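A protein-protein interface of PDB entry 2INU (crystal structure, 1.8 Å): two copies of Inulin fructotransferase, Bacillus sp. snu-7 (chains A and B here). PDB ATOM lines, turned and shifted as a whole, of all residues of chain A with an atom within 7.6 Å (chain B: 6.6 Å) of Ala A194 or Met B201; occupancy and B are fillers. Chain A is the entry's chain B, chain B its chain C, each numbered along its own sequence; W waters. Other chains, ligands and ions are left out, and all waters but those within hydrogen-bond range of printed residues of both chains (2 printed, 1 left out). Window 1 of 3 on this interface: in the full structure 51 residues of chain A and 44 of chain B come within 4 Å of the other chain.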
ATOM      1  N   ARG A 134      -7.882   8.802  11.049  1.00  0.00           N
ATOM      2  CA  ARG A 134      -8.292   8.567   9.689  1.00  0.00           C
ATOM      3  C   ARG A 134      -9.488   9.460   9.571  1.00  0.00           C
ATOM      4  O   ARG A 134     -10.149   9.766  10.565  1.00  0.00           O
ATOM      5  CB  ARG A 134      -8.773   7.161   9.443  1.00  0.00           C
ATOM      6  CG  ARG A 134      -7.762   6.068   9.621  1.00  0.00           C
ATOM      7  CD  ARG A 134      -8.530   4.761   9.512  1.00  0.00           C
ATOM      8  NE  ARG A 134      -9.379   4.558  10.684  1.00  0.00           N
ATOM      9  CZ  ARG A 134     -10.221   3.547  10.826  1.00  0.00           C
ATOM     10  NH1 ARG A 134     -10.343   2.642   9.871  1.00  0.00           N
ATOM     11  NH2 ARG A 134     -10.929   3.433  11.931  1.00  0.00           N
ATOM     12  N   ASN A 170     -10.516   5.557   5.610  1.00  0.00           N
ATOM     13  CA  ASN A 170     -11.649   6.313   6.099  1.00  0.00           C
ATOM     14  C   ASN A 170     -12.543   5.514   7.031  1.00  0.00           C
ATOM     15  O   ASN A 170     -12.537   4.280   7.024  1.00  0.00           O
ATOM     16  CB  ASN A 170     -12.476   6.747   4.901  1.00  0.00           C
ATOM     17  CG  ASN A 170     -12.824   5.573   3.996  1.00  0.00           C
ATOM     18  OD1 ASN A 170     -13.909   5.006   4.088  1.00  0.00           O
ATOM     19  ND2 ASN A 170     -11.886   5.189   3.135  1.00  0.00           N
ATOM     20  N   ASP A 171     -13.308   6.219   7.854  1.00  0.00           N
ATOM     21  CA  ASP A 171     -14.225   5.525   8.734  1.00  0.00           C
ATOM     22  C   ASP A 171     -15.584   6.191   8.779  1.00  0.00           C
ATOM     23  O   ASP A 171     -15.711   7.413   8.835  1.00  0.00           O
ATOM     24  CB  ASP A 171     -13.669   5.403  10.147  1.00  0.00           C
ATOM     25  CG  ASP A 171     -14.531   4.518  11.017  1.00  0.00           C
ATOM     26  OD1 ASP A 171     -15.063   3.513  10.486  1.00  0.00           O
ATOM     27  OD2 ASP A 171     -14.683   4.800  12.229  1.00  0.00           O
ATOM     28  N   SER A 172     -16.598   5.341   8.710  1.00  0.00           N
ATOM     29  CA  SER A 172     -17.996   5.734   8.754  1.00  0.00           C
ATOM     30  C   SER A 172     -18.426   6.727   7.675  1.00  0.00           C
ATOM     31  O   SER A 172     -19.222   7.625   7.939  1.00  0.00           O
ATOM     32  CB  SER A 172     -18.329   6.303  10.130  1.00  0.00           C
ATOM     33  OG  SER A 172     -19.715   6.184  10.387  1.00  0.00           O
ATOM     34  N   PHE A 173     -17.918   6.572   6.459  1.00  0.00           N
ATOM     35  CA  PHE A 173     -18.322   7.480   5.395  1.00  0.00           C
ATOM     36  C   PHE A 173     -19.741   7.125   4.985  1.00  0.00           C
ATOM     37  O   PHE A 173     -20.172   5.976   5.155  1.00  0.00           O
ATOM     38  CB  PHE A 173     -17.365   7.386   4.205  1.00  0.00           C
ATOM     39  CG  PHE A 173     -16.152   8.279   4.338  1.00  0.00           C
ATOM     40  CD1 PHE A 173     -15.639   8.590   5.591  1.00  0.00           C
ATOM     41  CD2 PHE A 173     -15.511   8.780   3.219  1.00  0.00           C
ATOM     42  CE1 PHE A 173     -14.508   9.385   5.726  1.00  0.00           C
ATOM     43  CE2 PHE A 173     -14.378   9.576   3.339  1.00  0.00           C
ATOM     44  CZ  PHE A 173     -13.866   9.884   4.595  1.00  0.00           C
ATOM     45  N   HIS A 174     -20.463   8.107   4.453  1.00  0.00           N
ATOM     46  CA  HIS A 174     -21.847   7.914   4.034  1.00  0.00           C
ATOM     47  C   HIS A 174     -22.050   8.564   2.669  1.00  0.00           C
ATOM     48  O   HIS A 174     -21.768   9.749   2.483  1.00  0.00           O
ATOM     49  CB  HIS A 174     -22.785   8.555   5.063  1.00  0.00           C
ATOM     50  CG  HIS A 174     -24.213   8.163   4.915  1.00  0.00           C
ATOM     51  ND1 HIS A 174     -24.651   7.212   4.014  1.00  0.00           N
ATOM     52  CD2 HIS A 174     -25.326   8.581   5.580  1.00  0.00           C
ATOM     53  CE1 HIS A 174     -25.957   7.067   4.128  1.00  0.00           C
ATOM     54  NE2 HIS A 174     -26.388   7.882   5.066  1.00  0.00           N
ATOM     55  N   GLY A 191      -9.782   1.440   1.254  1.00  0.00           N
ATOM     56  CA  GLY A 191      -9.718   1.309   2.699  1.00  0.00           C
ATOM     57  C   GLY A 191     -10.989   1.706   3.422  1.00  0.00           C
ATOM     58  O   GLY A 191     -10.940   2.324   4.490  1.00  0.00           O
ATOM     59  N   ALA A 192     -12.129   1.353   2.834  1.00  0.00           N
ATOM     60  CA  ALA A 192     -13.429   1.670   3.412  1.00  0.00           C
ATOM     61  C   ALA A 192     -13.679   0.809   4.642  1.00  0.00           C
ATOM     62  O   ALA A 192     -13.401  -0.392   4.650  1.00  0.00           O
ATOM     63  CB  ALA A 192     -14.521   1.453   2.388  1.00  0.00           C
ATOM     64  N   ASP A 193     -14.209   1.444   5.678  1.00  0.00           N
ATOM     65  CA  ASP A 193     -14.487   0.793   6.947  1.00  0.00           C
ATOM     66  C   ASP A 193     -15.801   1.387   7.474  1.00  0.00           C
ATOM     67  O   ASP A 193     -15.901   2.594   7.693  1.00  0.00           O
ATOM     68  CB  ASP A 193     -13.292   1.069   7.869  1.00  0.00           C
ATOM     69  CG  ASP A 193     -13.546   0.702   9.316  1.00  0.00           C
ATOM     70  OD1 ASP A 193     -14.266  -0.287   9.585  1.00  0.00           O
ATOM     71  OD2 ASP A 193     -13.001   1.400  10.205  1.00  0.00           O
ATOM     72  N   ALA A 194     -16.805   0.527   7.643  1.00  0.00           N
ATOM     73  CA  ALA A 194     -18.133   0.928   8.108  1.00  0.00           C
ATOM     74  C   ALA A 194     -18.746   1.907   7.118  1.00  0.00           C
ATOM     75  O   ALA A 194     -19.546   2.773   7.494  1.00  0.00           O
ATOM     76  CB  ALA A 194     -18.048   1.562   9.488  1.00  0.00           C
ATOM     77  N   LEU A 195     -18.349   1.763   5.857  1.00  0.00           N
ATOM     78  CA  LEU A 195     -18.851   2.608   4.792  1.00  0.00           C
ATOM     79  C   LEU A 195     -20.278   2.269   4.448  1.00  0.00           C
ATOM     80  O   LEU A 195     -20.724   1.130   4.595  1.00  0.00           O
ATOM     81  CB  LEU A 195     -18.007   2.457   3.520  1.00  0.00           C
ATOM     82  CG  LEU A 195     -18.641   3.067   2.260  1.00  0.00           C
ATOM     83  CD1 LEU A 195     -18.671   4.578   2.373  1.00  0.00           C
ATOM     84  CD2 LEU A 195     -17.858   2.644   1.031  1.00  0.00           C
ATOM     85  N   ARG A 196     -20.994   3.274   3.978  1.00  0.00           N
ATOM     86  CA  ARG A 196     -22.356   3.049   3.574  1.00  0.00           C
ATOM     87  C   ARG A 196     -22.659   3.770   2.291  1.00  0.00           C
ATOM     88  O   ARG A 196     -22.539   4.991   2.190  1.00  0.00           O
ATOM     89  CB  ARG A 196     -23.327   3.493   4.641  1.00  0.00           C
ATOM     90  CG  ARG A 196     -24.747   3.206   4.264  1.00  0.00           C
ATOM     91  CD  ARG A 196     -25.633   3.861   5.256  1.00  0.00           C
ATOM     92  NE  ARG A 196     -25.433   3.248   6.559  1.00  0.00           N
ATOM     93  CZ  ARG A 196     -25.242   3.940   7.676  1.00  0.00           C
ATOM     94  NH1 ARG A 196     -25.219   5.270   7.644  1.00  0.00           N
ATOM     95  NH2 ARG A 196     -25.089   3.306   8.829  1.00  0.00           N
ATOM     96  N   VAL A 197     -23.038   2.967   1.312  1.00  0.00           N
ATOM     97  CA  VAL A 197     -23.390   3.418  -0.008  1.00  0.00           C
ATOM     98  C   VAL A 197     -24.806   2.884  -0.166  1.00  0.00           C
ATOM     99  O   VAL A 197     -25.012   1.677  -0.283  1.00  0.00           O
ATOM    100  CB  VAL A 197     -22.430   2.787  -1.035  1.00  0.00           C
ATOM    101  CG1 VAL A 197     -22.786   3.225  -2.435  1.00  0.00           C
ATOM    102  CG2 VAL A 197     -20.996   3.179  -0.706  1.00  0.00           C
ATOM    103  N   GLY A 215     -11.228  -3.619   2.969  1.00  0.00           N
ATOM    104  CA  GLY A 215     -12.377  -3.058   3.651  1.00  0.00           C
ATOM    105  C   GLY A 215     -12.972  -3.906   4.754  1.00  0.00           C
ATOM    106  O   GLY A 215     -12.690  -5.097   4.872  1.00  0.00           O
ATOM    107  N   GLN A 216     -13.818  -3.272   5.559  1.00  0.00           N
ATOM    108  CA  GLN A 216     -14.493  -3.934   6.657  1.00  0.00           C
ATOM    109  C   GLN A 216     -15.891  -3.372   6.885  1.00  0.00           C
ATOM    110  O   GLN A 216     -16.137  -2.186   6.685  1.00  0.00           O
ATOM    111  CB  GLN A 216     -13.690  -3.795   7.951  1.00  0.00           C
ATOM    112  CG  GLN A 216     -12.225  -4.167   7.856  1.00  0.00           C
ATOM    113  CD  GLN A 216     -11.752  -4.941   9.054  1.00  0.00           C
ATOM    114  OE1 GLN A 216     -12.058  -4.590  10.204  1.00  0.00           O
ATOM    115  NE2 GLN A 216     -10.972  -5.993   8.799  1.00  0.00           N
ATOM    116  N   ALA A 217     -16.791  -4.255   7.311  1.00  0.00           N
ATOM    117  CA  ALA A 217     -18.187  -3.937   7.603  1.00  0.00           C
ATOM    118  C   ALA A 217     -18.762  -2.798   6.769  1.00  0.00           C
ATOM    119  O   ALA A 217     -19.177  -1.768   7.292  1.00  0.00           O
ATOM    120  CB  ALA A 217     -18.344  -3.630   9.069  1.00  0.00           C
ATOM    121  N   THR A 218     -18.816  -3.014   5.465  1.00  0.00           N
ATOM    122  CA  THR A 218     -19.344  -2.036   4.539  1.00  0.00           C
ATOM    123  C   THR A 218     -20.728  -2.496   4.090  1.00  0.00           C
ATOM    124  O   THR A 218     -20.999  -3.689   4.022  1.00  0.00           O
ATOM    125  CB  THR A 218     -18.406  -1.896   3.319  1.00  0.00           C
ATOM    126  OG1 THR A 218     -17.193  -1.248   3.733  1.00  0.00           O
ATOM    127  CG2 THR A 218     -19.070  -1.082   2.224  1.00  0.00           C
ATOM    128  N   ILE A 219     -21.601  -1.541   3.797  1.00  0.00           N
ATOM    129  CA  ILE A 219     -22.946  -1.844   3.340  1.00  0.00           C
ATOM    130  C   ILE A 219     -23.244  -1.131   2.039  1.00  0.00           C
ATOM    131  O   ILE A 219     -23.061   0.084   1.930  1.00  0.00           O
ATOM    132  CB  ILE A 219     -24.021  -1.414   4.366  1.00  0.00           C
ATOM    133  CG1 ILE A 219     -23.763  -2.073   5.727  1.00  0.00           C
ATOM    134  CG2 ILE A 219     -25.396  -1.790   3.844  1.00  0.00           C
ATOM    135  CD1 ILE A 219     -24.721  -1.616   6.800  1.00  0.00           C
ATOM    136  N   HIS A 239     -12.177  -7.374   0.930  1.00  0.00           N
ATOM    137  CA  HIS A 239     -13.173  -6.904   1.874  1.00  0.00           C
ATOM    138  C   HIS A 239     -13.611  -8.050   2.747  1.00  0.00           C
ATOM    139  O   HIS A 239     -13.599  -9.215   2.338  1.00  0.00           O
ATOM    140  CB  HIS A 239     -14.396  -6.322   1.162  1.00  0.00           C
ATOM    141  CG  HIS A 239     -14.370  -4.841   1.035  1.00  0.00           C
ATOM    142  ND1 HIS A 239     -15.273  -4.013   1.654  1.00  0.00           N
ATOM    143  CD2 HIS A 239     -13.532  -4.011   0.335  1.00  0.00           C
ATOM    144  CE1 HIS A 239     -15.013  -2.751   1.353  1.00  0.00           C
ATOM    145  NE2 HIS A 239     -13.960  -2.736   0.555  1.00  0.00           N
ATOM    146  N   HIS B  87     -23.945  12.430  11.014  1.00  0.00           N
ATOM    147  CA  HIS B  87     -23.863  11.467  12.117  1.00  0.00           C
ATOM    148  C   HIS B  87     -22.540  11.616  12.867  1.00  0.00           C
ATOM    149  O   HIS B  87     -22.394  11.163  13.999  1.00  0.00           O
ATOM    150  CB  HIS B  87     -23.988  10.038  11.572  1.00  0.00           C
ATOM    151  CG  HIS B  87     -22.886   9.647  10.649  1.00  0.00           C
ATOM    152  ND1 HIS B  87     -22.642  10.290   9.449  1.00  0.00           N
ATOM    153  CD2 HIS B  87     -21.944   8.667  10.736  1.00  0.00           C
ATOM    154  CE1 HIS B  87     -21.610   9.725   8.847  1.00  0.00           C
ATOM    155  NE2 HIS B  87     -21.173   8.745   9.606  1.00  0.00           N
ATOM    156  N   PHE B  89     -19.748  10.165  13.274  1.00  0.00           N
ATOM    157  CA  PHE B  89     -19.136   9.160  14.126  1.00  0.00           C
ATOM    158  C   PHE B  89     -17.617   9.273  14.139  1.00  0.00           C
ATOM    159  O   PHE B  89     -16.981   9.686  13.155  1.00  0.00           O
ATOM    160  CB  PHE B  89     -19.530   7.742  13.718  1.00  0.00           C
ATOM    161  CG  PHE B  89     -18.920   6.679  14.601  1.00  0.00           C
ATOM    162  CD1 PHE B  89     -17.709   6.090  14.267  1.00  0.00           C
ATOM    163  CD2 PHE B  89     -19.532   6.317  15.804  1.00  0.00           C
ATOM    164  CE1 PHE B  89     -17.108   5.162  15.112  1.00  0.00           C
ATOM    165  CE2 PHE B  89     -18.943   5.390  16.657  1.00  0.00           C
ATOM    166  CZ  PHE B  89     -17.724   4.816  16.303  1.00  0.00           C
ATOM    167  N   GLY B 177     -30.271   8.081   9.972  1.00  0.00           N
ATOM    168  CA  GLY B 177     -29.050   8.836   9.727  1.00  0.00           C
ATOM    169  C   GLY B 177     -28.288   9.294  10.950  1.00  0.00           C
ATOM    170  O   GLY B 177     -27.396  10.128  10.860  1.00  0.00           O
ATOM    171  N   MET B 178     -28.612   8.723  12.099  1.00  0.00           N
ATOM    172  CA  MET B 178     -27.977   9.115  13.349  1.00  0.00           C
ATOM    173  C   MET B 178     -26.600   8.540  13.647  1.00  0.00           C
ATOM    174  O   MET B 178     -26.144   7.585  13.014  1.00  0.00           O
ATOM    175  CB  MET B 178     -28.910   8.788  14.498  1.00  0.00           C
ATOM    176  CG  MET B 178     -30.258   9.436  14.356  1.00  0.00           C
ATOM    177  SD  MET B 178     -30.210  11.188  15.072  1.00  0.00           S
ATOM    178  CE  MET B 178     -29.653  10.713  16.810  1.00  0.00           C
ATOM    179  N   GLY B 179     -25.946   9.158  14.625  1.00  0.00           N
ATOM    180  CA  GLY B 179     -24.628   8.742  15.051  1.00  0.00           C
ATOM    181  C   GLY B 179     -24.661   8.686  16.562  1.00  0.00           C
ATOM    182  O   GLY B 179     -24.856   9.704  17.223  1.00  0.00           O
ATOM    183  N   PHE B 180     -24.500   7.489  17.114  1.00  0.00           N
ATOM    184  CA  PHE B 180     -24.501   7.300  18.562  1.00  0.00           C
ATOM    185  C   PHE B 180     -23.129   6.774  18.927  1.00  0.00           C
ATOM    186  O   PHE B 180     -22.638   5.839  18.292  1.00  0.00           O
ATOM    187  CB  PHE B 180     -25.546   6.258  18.978  1.00  0.00           C
ATOM    188  CG  PHE B 180     -26.966   6.672  18.717  1.00  0.00           C
ATOM    189  CD1 PHE B 180     -27.732   7.280  19.716  1.00  0.00           C
ATOM    190  CD2 PHE B 180     -27.563   6.392  17.496  1.00  0.00           C
ATOM    191  CE1 PHE B 180     -29.067   7.589  19.499  1.00  0.00           C
ATOM    192  CE2 PHE B 180     -28.898   6.699  17.276  1.00  0.00           C
ATOM    193  CZ  PHE B 180     -29.652   7.292  18.272  1.00  0.00           C
ATOM    194  N   VAL B 181     -22.516   7.341  19.958  1.00  0.00           N
ATOM    195  CA  VAL B 181     -21.209   6.863  20.360  1.00  0.00           C
ATOM    196  C   VAL B 181     -20.913   7.084  21.841  1.00  0.00           C
ATOM    197  O   VAL B 181     -21.251   8.120  22.412  1.00  0.00           O
ATOM    198  CB  VAL B 181     -20.111   7.500  19.476  1.00  0.00           C
ATOM    199  CG1 VAL B 181     -20.096   9.011  19.641  1.00  0.00           C
ATOM    200  CG2 VAL B 181     -18.755   6.909  19.820  1.00  0.00           C
ATOM    201  N   ASP B 199     -30.577   3.074   8.519  1.00  0.00           N
ATOM    202  CA  ASP B 199     -29.453   3.893   8.071  1.00  0.00           C
ATOM    203  C   ASP B 199     -28.744   4.637   9.223  1.00  0.00           C
ATOM    204  O   ASP B 199     -28.354   5.795   9.065  1.00  0.00           O
ATOM    205  CB  ASP B 199     -29.947   4.916   7.042  1.00  0.00           C
ATOM    206  CG  ASP B 199     -28.855   5.368   6.101  1.00  0.00           C
ATOM    207  OD1 ASP B 199     -27.703   5.570   6.552  1.00  0.00           O
ATOM    208  OD2 ASP B 199     -29.145   5.527   4.895  1.00  0.00           O
ATOM    209  N   ASN B 200     -28.573   3.977  10.369  1.00  0.00           N
ATOM    210  CA  ASN B 200     -27.894   4.591  11.508  1.00  0.00           C
ATOM    211  C   ASN B 200     -26.572   3.928  11.846  1.00  0.00           C
ATOM    212  O   ASN B 200     -26.351   2.756  11.544  1.00  0.00           O
ATOM    213  CB  ASN B 200     -28.771   4.568  12.774  1.00  0.00           C
ATOM    214  CG  ASN B 200     -30.152   5.133  12.546  1.00  0.00           C
ATOM    215  OD1 ASN B 200     -30.300   6.437  12.747  1.00  0.00           O
ATOM    216  ND2 ASN B 200     -31.081   4.402  12.201  1.00  0.00           N
ATOM    217  N   MET B 201     -25.706   4.703  12.494  1.00  0.00           N
ATOM    218  CA  MET B 201     -24.400   4.236  12.945  1.00  0.00           C
ATOM    219  C   MET B 201     -24.399   4.302  14.463  1.00  0.00           C
ATOM    220  O   MET B 201     -24.234   5.380  15.049  1.00  0.00           O
ATOM    221  CB  MET B 201     -23.283   5.109  12.367  1.00  0.00           C
ATOM    222  CG  MET B 201     -21.914   4.865  12.970  1.00  0.00           C
ATOM    223  SD  MET B 201     -21.257   3.090  12.683  1.00  0.00           S
ATOM    224  CE  MET B 201     -19.494   3.544  12.079  1.00  0.00           C
ATOM    225  N   ILE B 202     -24.603   3.145  15.085  1.00  0.00           N
ATOM    226  CA  ILE B 202     -24.674   3.032  16.535  1.00  0.00           C
ATOM    227  C   ILE B 202     -23.555   2.105  16.999  1.00  0.00           C
ATOM    228  O   ILE B 202     -23.680   0.875  16.885  1.00  0.00           O
ATOM    229  CB  ILE B 202     -26.000   2.393  16.939  1.00  0.00           C
ATOM    230  CG1 ILE B 202     -27.129   3.003  16.104  1.00  0.00           C
ATOM    231  CG2 ILE B 202     -26.259   2.604  18.424  1.00  0.00           C
ATOM    232  CD1 ILE B 202     -28.452   2.309  16.244  1.00  0.00           C
ATOM    233  N   ALA B 203     -22.475   2.662  17.533  1.00  0.00           N
ATOM    234  CA  ALA B 203     -21.389   1.801  17.971  1.00  0.00           C
ATOM    235  C   ALA B 203     -20.576   2.358  19.119  1.00  0.00           C
ATOM    236  O   ALA B 203     -20.591   3.570  19.391  1.00  0.00           O
ATOM    237  CB  ALA B 203     -20.482   1.485  16.797  1.00  0.00           C
ATOM    238  N   GLY B 222     -30.640  -1.540   7.372  1.00  0.00           N
ATOM    239  CA  GLY B 222     -29.551  -0.676   6.938  1.00  0.00           C
ATOM    240  C   GLY B 222     -28.697  -0.042   8.028  1.00  0.00           C
ATOM    241  O   GLY B 222     -28.009   0.954   7.779  1.00  0.00           O
ATOM    242  N   ASN B 223     -28.709  -0.626   9.225  1.00  0.00           N
ATOM    243  CA  ASN B 223     -27.933  -0.089  10.337  1.00  0.00           C
ATOM    244  C   ASN B 223     -26.573  -0.761  10.560  1.00  0.00           C
ATOM    245  O   ASN B 223     -26.365  -1.923  10.202  1.00  0.00           O
ATOM    246  CB  ASN B 223     -28.729  -0.187  11.638  1.00  0.00           C
ATOM    247  CG  ASN B 223     -30.095   0.468  11.546  1.00  0.00           C
ATOM    248  OD1 ASN B 223     -30.116   1.795  11.556  1.00  0.00           O
ATOM    249  ND2 ASN B 223     -31.119  -0.211  11.459  1.00  0.00           N
ATOM    250  N   HIS B 224     -25.659   0.002  11.164  1.00  0.00           N
ATOM    251  CA  HIS B 224     -24.296  -0.432  11.514  1.00  0.00           C
ATOM    252  C   HIS B 224     -24.244  -0.461  13.044  1.00  0.00           C
ATOM    253  O   HIS B 224     -24.269   0.607  13.665  1.00  0.00           O
ATOM    254  CB  HIS B 224     -23.264   0.610  11.057  1.00  0.00           C
ATOM    255  CG  HIS B 224     -22.777   0.448   9.653  1.00  0.00           C
ATOM    256  ND1 HIS B 224     -21.947  -0.573   9.244  1.00  0.00           N
ATOM    257  CD2 HIS B 224     -22.925   1.250   8.548  1.00  0.00           C
ATOM    258  CE1 HIS B 224     -21.602  -0.405   7.978  1.00  0.00           C
ATOM    259  NE2 HIS B 224     -22.184   0.695   7.543  1.00  0.00           N
ATOM    260  N   MET B 225     -24.175  -1.631  13.678  1.00  0.00           N
ATOM    261  CA  MET B 225     -24.142  -1.637  15.156  1.00  0.00           C
ATOM    262  C   MET B 225     -23.055  -2.480  15.833  1.00  0.00           C
ATOM    263  O   MET B 225     -22.712  -3.588  15.390  1.00  0.00           O
ATOM    264  CB  MET B 225     -25.469  -2.114  15.740  1.00  0.00           C
ATOM    265  CG  MET B 225     -26.677  -1.231  15.462  1.00  0.00           C
ATOM    266  SD  MET B 225     -28.226  -2.144  16.160  1.00  0.00           S
ATOM    267  CE  MET B 225     -29.460  -1.784  14.706  1.00  0.00           C
ATOM    268  N   PHE B 250     -21.547  -5.758  14.093  1.00  0.00           N
ATOM    269  CA  PHE B 250     -20.195  -6.181  14.384  1.00  0.00           C
ATOM    270  C   PHE B 250     -19.899  -6.235  15.874  1.00  0.00           C
ATOM    271  O   PHE B 250     -20.741  -5.895  16.708  1.00  0.00           O
ATOM    272  CB  PHE B 250     -19.226  -5.249  13.661  1.00  0.00           C
ATOM    273  CG  PHE B 250     -19.641  -3.806  13.705  1.00  0.00           C
ATOM    274  CD1 PHE B 250     -19.446  -3.053  14.856  1.00  0.00           C
ATOM    275  CD2 PHE B 250     -20.250  -3.206  12.608  1.00  0.00           C
ATOM    276  CE1 PHE B 250     -19.844  -1.723  14.916  1.00  0.00           C
ATOM    277  CE2 PHE B 250     -20.655  -1.878  12.653  1.00  0.00           C
ATOM    278  CZ  PHE B 250     -20.455  -1.134  13.803  1.00  0.00           C
HETATM  279  O   HOH W   1     -21.310   3.939   9.541  1.00  0.00           O
HETATM  280  O   HOH W   2     -28.043   2.006   5.127  1.00  0.00           O
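O of Ser A172 lies within hydrogen-bond range of NE2 of His B87, at 2.8 Å.
OD1 of Asp B199 is in hydrogen-bond range of NE2 of His A174 (3.0 Å).
O of Ala A194 is in hydrogen-bond range of NE2 of His B224 (3.4 Å).
The backbone carbonyl oxygen (O) of Leu A195 sits at hydrogen-bond distance from a ring nitrogen (NE2) of His B224 (3.3 Å).
The guanidinium group of Arg A196 lies within salt-bridge range of the side-chain carboxylate of Asp B199.
The backbone carbonyl oxygen (O) of Asn B200 sits at hydrogen-bond distance from the guanidinium group (NH2) of Arg A196 (3.0 Å).
The backbone NH (N) of Ala A194 lies within hydrogen-bond range of the backbone carbonyl oxygen (O) of Gln A216, 3.0 Å away.
The backbone NH (N) of Ala A194 lies close to the backbone carbonyl oxygen (O) of Ala A217.
The backbone NH of Gly B177 is in hydrogen-bond range of the backbone carbonyl oxygen of Asp B199 (3.1 Å).
OD1 of Asn B223 is in hydrogen-bond range of N of Asp B199.
The backbone NH (N) of His B224 is in hydrogen-bond range of the backbone carbonyl oxygen (O) of Asn B200 (2.9 Å).
The backbone carbonyl oxygen (O) of His B224 is in hydrogen-bond range of the backbone NH (N) of Ile B202 (2.9 Å).
Asp A171 touches Phe B89.
CB of Phe B89 touches OG of Ser A172, at 3.7 Å.
Ser A172 touches Met B201.
CE of Met B201 touches CB of Ala A194 (3.6 Å).
Arg A196 touches Met B201.
NE of Arg A196 touches O of Gly B222 (3.7 Å).
His B224 touches Arg A196.
O of Ala A217 touches CE1 of His B224 (2.9 Å).
Ile A219 touches Asn B223 (CD1 to O, 3.8 Å).
Ile A219 touches His B224.
Printed residues of chain A within 4 Å of Asn B200: Arg A196.
Of the printed residues of chain B, Leu A195 touches His B224.
Of the printed residues of chain B, His A174 touches Asp B199 (3.0 Å).
Printed residues of chain A within 4 Å of Phe B89: Asp A171 (3.8 Å) and Ser A172 (3.7 Å).
Printed residues of chain B within 4 Å of Arg A196: Asp B199, Asn B200, Met B201, Gly B222 and His B224.
Met B225 touches none of the printed residues of chain A.
Ala A192 touches none of the printed residues of chain B.
The nearest residue of chain A that does not touch Met B201 is Asp A171 (4.7 Å).
Of the 17 printed residues of chain B, 8 touch a printed residue of chain A.
Hydrophobic or aromatic side chains of chain B that line the printed part of chain A: His B87, Phe B89, Met B201 and His B224.
Printed residues of chain A that touch a printed residue of chain B: Asp A171, Ser A172, His A174, Ala A194, Leu A195, Arg A196, Ala A217 and Ile A219.
Along chain A the printed residues that touch a printed residue of chain B span positions 171 to 219.
Among the printed residues, Asp or Glu carboxylates within 4 Å of a Lys or Arg side-chain nitrogen of the other chain: Arg A196 with Asp B199 (2.7 Å).
No position is printed for both chains.
Of the 16 pairs that touch across the chains among the printed residues, none has its exchanged pair printed and touching as well.
Water W2 lies within hydrogen-bond range of the backbone carbonyl oxygen of Gly B222 (2.9 Å) and the guanidinium group of Arg A196 (3.2 Å).
Water W1 lies within hydrogen-bond range of the side-chain hydroxyl of Ser A172, the backbone carbonyl oxygen of Ala A194 and the side-chain sulfur of Met B201.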
